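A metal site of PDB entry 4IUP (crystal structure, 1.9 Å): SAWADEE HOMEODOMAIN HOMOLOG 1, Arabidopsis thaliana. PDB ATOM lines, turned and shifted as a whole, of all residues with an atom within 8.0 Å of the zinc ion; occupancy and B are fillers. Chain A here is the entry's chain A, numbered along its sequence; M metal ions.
Of the 20 residues printed, 4 come within 4 Å of the zinc ion.
The nearest printed residue that does not touch the zinc ion is Arg 99 (4.3 Å).
SG of Cys 109 binds the zinc ion.
SG of Cys 68 is bound to the zinc ion, at 2.4 Å.
SG of Cys 107 is bound to the zinc ion.
A ring nitrogen (NE2) of His 102 is bound to the zinc ion (2.5 Å).
ND1 of His 102 sits at hydrogen-bond distance from O of Arg 106 (3.0 Å).
The backbone carbonyl oxygen (O) of Pro 65 lies close to the side-chain sulfur (SG) of Cys 68 (3.7 Å).
O of Cys 68 lies within hydrogen-bond range of NH1 of Arg 99.
SG of Cys 109 lies close to N of Gly 100, 3.4 Å away.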
ATOM      1  N   GLU A  64       9.694  33.513  19.545  1.00  0.00           N
ATOM      2  CA  GLU A  64       8.796  34.276  20.419  1.00  0.00           C
ATOM      3  C   GLU A  64       7.372  33.703  20.368  1.00  0.00           C
ATOM      4  O   GLU A  64       6.963  33.152  19.348  1.00  0.00           O
ATOM      5  CB  GLU A  64       8.807  35.757  20.042  1.00  0.00           C
ATOM      6  CG  GLU A  64      10.161  36.462  20.225  1.00  0.00           C
ATOM      7  CD  GLU A  64      10.726  36.343  21.649  1.00  0.00           C
ATOM      8  OE1 GLU A  64       9.968  36.585  22.620  1.00  0.00           O
ATOM      9  OE2 GLU A  64      11.926  36.003  21.786  1.00  0.00           O
ATOM     10  N   PRO A  65       6.604  33.844  21.463  1.00  0.00           N
ATOM     11  CA  PRO A  65       5.260  33.240  21.475  1.00  0.00           C
ATOM     12  C   PRO A  65       4.385  33.632  20.282  1.00  0.00           C
ATOM     13  O   PRO A  65       3.654  32.788  19.761  1.00  0.00           O
ATOM     14  CB  PRO A  65       4.664  33.737  22.792  1.00  0.00           C
ATOM     15  CG  PRO A  65       5.861  33.940  23.673  1.00  0.00           C
ATOM     16  CD  PRO A  65       6.934  34.465  22.769  1.00  0.00           C
ATOM     17  N   SER A  66       4.480  34.891  19.835  1.00  0.00           N
ATOM     18  CA  SER A  66       3.656  35.392  18.729  1.00  0.00           C
ATOM     19  C   SER A  66       3.992  34.759  17.374  1.00  0.00           C
ATOM     20  O   SER A  66       3.237  34.894  16.408  1.00  0.00           O
ATOM     21  CB  SER A  66       3.771  36.913  18.622  1.00  0.00           C
ATOM     22  OG  SER A  66       5.085  37.293  18.259  1.00  0.00           O
ATOM     23  N   GLU A  67       5.140  34.075  17.303  1.00  0.00           N
ATOM     24  CA  GLU A  67       5.562  33.422  16.065  1.00  0.00           C
ATOM     25  C   GLU A  67       5.661  31.888  16.165  1.00  0.00           C
ATOM     26  O   GLU A  67       6.327  31.261  15.337  1.00  0.00           O
ATOM     27  CB  GLU A  67       6.881  34.017  15.559  1.00  0.00           C
ATOM     28  CG  GLU A  67       8.025  33.953  16.558  1.00  0.00           C
ATOM     29  CD  GLU A  67       9.335  34.552  16.055  1.00  0.00           C
ATOM     30  OE1 GLU A  67       9.418  34.924  14.857  1.00  0.00           O
ATOM     31  OE2 GLU A  67      10.277  34.655  16.864  1.00  0.00           O
ATOM     32  N   CYS A  68       4.997  31.288  17.152  1.00  0.00           N
ATOM     33  CA  CYS A  68       5.055  29.828  17.326  1.00  0.00           C
ATOM     34  C   CYS A  68       4.442  29.080  16.144  1.00  0.00           C
ATOM     35  O   CYS A  68       4.664  27.879  15.993  1.00  0.00           O
ATOM     36  CB  CYS A  68       4.394  29.401  18.638  1.00  0.00           C
ATOM     37  SG  CYS A  68       2.586  29.476  18.639  1.00  0.00           S
ATOM     38  N   GLY A  69       3.679  29.791  15.310  1.00  0.00           N
ATOM     39  CA  GLY A  69       3.116  29.190  14.098  1.00  0.00           C
ATOM     40  C   GLY A  69       4.154  28.841  13.049  1.00  0.00           C
ATOM     41  O   GLY A  69       3.883  28.029  12.149  1.00  0.00           O
ATOM     42  N   ILE A  97       2.578  18.531  16.992  1.00  0.00           N
ATOM     43  CA  ILE A  97       2.329  19.771  17.735  1.00  0.00           C
ATOM     44  C   ILE A  97       0.894  19.803  18.255  1.00  0.00           C
ATOM     45  O   ILE A  97      -0.055  19.721  17.473  1.00  0.00           O
ATOM     46  CB  ILE A  97       2.592  21.035  16.889  1.00  0.00           C
ATOM     47  CG1 ILE A  97       4.005  21.004  16.279  1.00  0.00           C
ATOM     48  CG2 ILE A  97       2.406  22.323  17.724  1.00  0.00           C
ATOM     49  CD1 ILE A  97       4.229  22.033  15.194  1.00  0.00           C
ATOM     50  N   LYS A  98       0.748  19.902  19.572  1.00  0.00           N
ATOM     51  CA  LYS A  98      -0.534  20.150  20.194  1.00  0.00           C
ATOM     52  C   LYS A  98      -0.658  21.658  20.434  1.00  0.00           C
ATOM     53  O   LYS A  98       0.018  22.205  21.296  1.00  0.00           O
ATOM     54  CB  LYS A  98      -0.655  19.385  21.504  1.00  0.00           C
ATOM     55  CG  LYS A  98      -2.087  19.077  21.943  1.00  0.00           C
ATOM     56  CD  LYS A  98      -2.130  18.351  23.288  1.00  0.00           C
ATOM     57  CE  LYS A  98      -1.154  17.160  23.368  1.00  0.00           C
ATOM     58  NZ  LYS A  98      -1.508  16.023  22.466  1.00  0.00           N
ATOM     59  N   ARG A  99      -1.513  22.304  19.643  1.00  0.00           N
ATOM     60  CA  ARG A  99      -1.646  23.758  19.666  1.00  0.00           C
ATOM     61  C   ARG A  99      -2.515  24.183  20.837  1.00  0.00           C
ATOM     62  O   ARG A  99      -3.574  23.602  21.076  1.00  0.00           O
ATOM     63  CB  ARG A  99      -2.225  24.283  18.349  1.00  0.00           C
ATOM     64  CG  ARG A  99      -1.319  24.123  17.133  1.00  0.00           C
ATOM     65  CD  ARG A  99      -0.096  25.040  17.206  1.00  0.00           C
ATOM     66  NE  ARG A  99       0.776  24.931  16.038  1.00  0.00           N
ATOM     67  CZ  ARG A  99       1.965  25.503  15.942  1.00  0.00           C
ATOM     68  NH1 ARG A  99       2.455  26.220  16.941  1.00  0.00           N
ATOM     69  NH2 ARG A  99       2.682  25.354  14.832  1.00  0.00           N
ATOM     70  N   GLY A 100      -2.064  25.193  21.572  1.00  0.00           N
ATOM     71  CA  GLY A 100      -2.806  25.697  22.729  1.00  0.00           C
ATOM     72  C   GLY A 100      -3.479  27.034  22.485  1.00  0.00           C
ATOM     73  O   GLY A 100      -3.261  27.675  21.455  1.00  0.00           O
ATOM     74  N   ILE A 101      -4.310  27.439  23.439  1.00  0.00           N
ATOM     75  CA  ILE A 101      -4.916  28.770  23.432  1.00  0.00           C
ATOM     76  C   ILE A 101      -4.015  29.713  24.224  1.00  0.00           C
ATOM     77  O   ILE A 101      -3.875  29.562  25.442  1.00  0.00           O
ATOM     78  CB  ILE A 101      -6.347  28.754  24.045  1.00  0.00           C
ATOM     79  CG1 ILE A 101      -7.251  27.787  23.278  1.00  0.00           C
ATOM     80  CG2 ILE A 101      -6.945  30.162  24.083  1.00  0.00           C
ATOM     81  CD1 ILE A 101      -8.483  27.323  24.066  1.00  0.00           C
ATOM     82  N   HIS A 102      -3.385  30.657  23.541  1.00  0.00           N
ATOM     83  CA  HIS A 102      -2.486  31.586  24.208  1.00  0.00           C
ATOM     84  C   HIS A 102      -2.298  32.874  23.420  1.00  0.00           C
ATOM     85  O   HIS A 102      -2.667  32.953  22.235  1.00  0.00           O
ATOM     86  CB  HIS A 102      -1.124  30.928  24.480  1.00  0.00           C
ATOM     87  CG  HIS A 102      -0.190  30.945  23.317  1.00  0.00           C
ATOM     88  ND1 HIS A 102       0.486  32.082  22.925  1.00  0.00           N
ATOM     89  CD2 HIS A 102       0.200  29.968  22.461  1.00  0.00           C
ATOM     90  CE1 HIS A 102       1.237  31.810  21.878  1.00  0.00           C
ATOM     91  NE2 HIS A 102       1.085  30.537  21.576  1.00  0.00           N
ATOM     92  N   ASP A 103      -1.725  33.875  24.082  1.00  0.00           N
ATOM     93  CA  ASP A 103      -1.459  35.173  23.460  1.00  0.00           C
ATOM     94  C   ASP A 103       0.041  35.359  23.222  1.00  0.00           C
ATOM     95  O   ASP A 103       0.794  34.393  23.158  1.00  0.00           O
ATOM     96  CB  ASP A 103      -2.051  36.326  24.292  1.00  0.00           C
ATOM     97  CG  ASP A 103      -1.381  36.511  25.658  1.00  0.00           C
ATOM     98  OD1 ASP A 103      -0.385  35.815  25.982  1.00  0.00           O
ATOM     99  OD2 ASP A 103      -1.845  37.378  26.431  1.00  0.00           O
ATOM    100  N   ARG A 106       3.191  34.164  26.266  1.00  0.00           N
ATOM    101  CA  ARG A 106       3.702  32.842  26.591  1.00  0.00           C
ATOM    102  C   ARG A 106       3.045  31.812  25.678  1.00  0.00           C
ATOM    103  O   ARG A 106       1.826  31.773  25.569  1.00  0.00           O
ATOM    104  CB  ARG A 106       3.371  32.496  28.042  1.00  0.00           C
ATOM    105  CG  ARG A 106       3.845  31.125  28.518  1.00  0.00           C
ATOM    106  CD  ARG A 106       5.210  31.251  29.128  1.00  0.00           C
ATOM    107  NE  ARG A 106       5.777  30.009  29.646  1.00  0.00           N
ATOM    108  CZ  ARG A 106       7.078  29.863  29.890  1.00  0.00           C
ATOM    109  NH1 ARG A 106       7.895  30.877  29.635  1.00  0.00           N
ATOM    110  NH2 ARG A 106       7.563  28.716  30.369  1.00  0.00           N
ATOM    111  N   CYS A 107       3.853  30.978  25.042  1.00  0.00           N
ATOM    112  CA  CYS A 107       3.322  29.890  24.241  1.00  0.00           C
ATOM    113  C   CYS A 107       3.110  28.655  25.116  1.00  0.00           C
ATOM    114  O   CYS A 107       3.998  28.284  25.877  1.00  0.00           O
ATOM    115  CB  CYS A 107       4.253  29.592  23.076  1.00  0.00           C
ATOM    116  SG  CYS A 107       3.862  28.089  22.156  1.00  0.00           S
ATOM    117  N   ASN A 108       1.916  28.058  25.012  1.00  0.00           N
ATOM    118  CA  ASN A 108       1.599  26.803  25.714  1.00  0.00           C
ATOM    119  C   ASN A 108       1.358  25.626  24.754  1.00  0.00           C
ATOM    120  O   ASN A 108       0.769  24.608  25.136  1.00  0.00           O
ATOM    121  CB  ASN A 108       0.422  26.979  26.697  1.00  0.00           C
ATOM    122  CG  ASN A 108      -0.884  27.384  26.023  1.00  0.00           C
ATOM    123  OD1 ASN A 108      -0.948  27.557  24.807  1.00  0.00           O
ATOM    124  ND2 ASN A 108      -1.937  27.532  26.836  1.00  0.00           N
ATOM    125  N   CYS A 109       1.804  25.775  23.502  1.00  0.00           N
ATOM    126  CA  CYS A 109       1.792  24.674  22.552  1.00  0.00           C
ATOM    127  C   CYS A 109       2.798  23.604  23.014  1.00  0.00           C
ATOM    128  O   CYS A 109       3.800  23.921  23.681  1.00  0.00           O
ATOM    129  CB  CYS A 109       2.120  25.157  21.140  1.00  0.00           C
ATOM    130  SG  CYS A 109       0.932  26.364  20.478  1.00  0.00           S
ATOM    131  N   VAL A 110       2.506  22.350  22.688  1.00  0.00           N
ATOM    132  CA  VAL A 110       3.381  21.229  23.057  1.00  0.00           C
ATOM    133  C   VAL A 110       3.985  20.599  21.804  1.00  0.00           C
ATOM    134  O   VAL A 110       3.267  20.127  20.923  1.00  0.00           O
ATOM    135  CB  VAL A 110       2.631  20.160  23.899  1.00  0.00           C
ATOM    136  CG1 VAL A 110       3.581  19.032  24.317  1.00  0.00           C
ATOM    137  CG2 VAL A 110       1.984  20.777  25.136  1.00  0.00           C
ATOM    138  N   PHE A 111       5.312  20.592  21.751  1.00  0.00           N
ATOM    139  CA  PHE A 111       6.044  20.093  20.587  1.00  0.00           C
ATOM    140  C   PHE A 111       6.684  18.765  20.952  1.00  0.00           C
ATOM    141  O   PHE A 111       7.562  18.722  21.823  1.00  0.00           O
ATOM    142  CB  PHE A 111       7.117  21.111  20.157  1.00  0.00           C
ATOM    143  CG  PHE A 111       6.567  22.498  19.883  1.00  0.00           C
ATOM    144  CD1 PHE A 111       6.197  22.865  18.592  1.00  0.00           C
ATOM    145  CD2 PHE A 111       6.429  23.420  20.914  1.00  0.00           C
ATOM    146  CE1 PHE A 111       5.680  24.139  18.320  1.00  0.00           C
ATOM    147  CE2 PHE A 111       5.919  24.700  20.662  1.00  0.00           C
ATOM    148  CZ  PHE A 111       5.544  25.060  19.361  1.00  0.00           C
ATOM    149  N   LEU A 126       7.818  25.711  23.851  1.00  0.00           N
ATOM    150  CA  LEU A 126       8.557  26.643  23.003  1.00  0.00           C
ATOM    151  C   LEU A 126       9.807  27.175  23.715  1.00  0.00           C
ATOM    152  O   LEU A 126      10.817  27.483  23.076  1.00  0.00           O
ATOM    153  CB  LEU A 126       7.668  27.822  22.575  1.00  0.00           C
ATOM    154  CG  LEU A 126       8.201  28.657  21.399  1.00  0.00           C
ATOM    155  CD1 LEU A 126       8.243  27.807  20.130  1.00  0.00           C
ATOM    156  CD2 LEU A 126       7.352  29.908  21.198  1.00  0.00           C
HETATM  157 ZN    ZN M   1       2.048  28.406  20.667  1.00  0.00          ZN
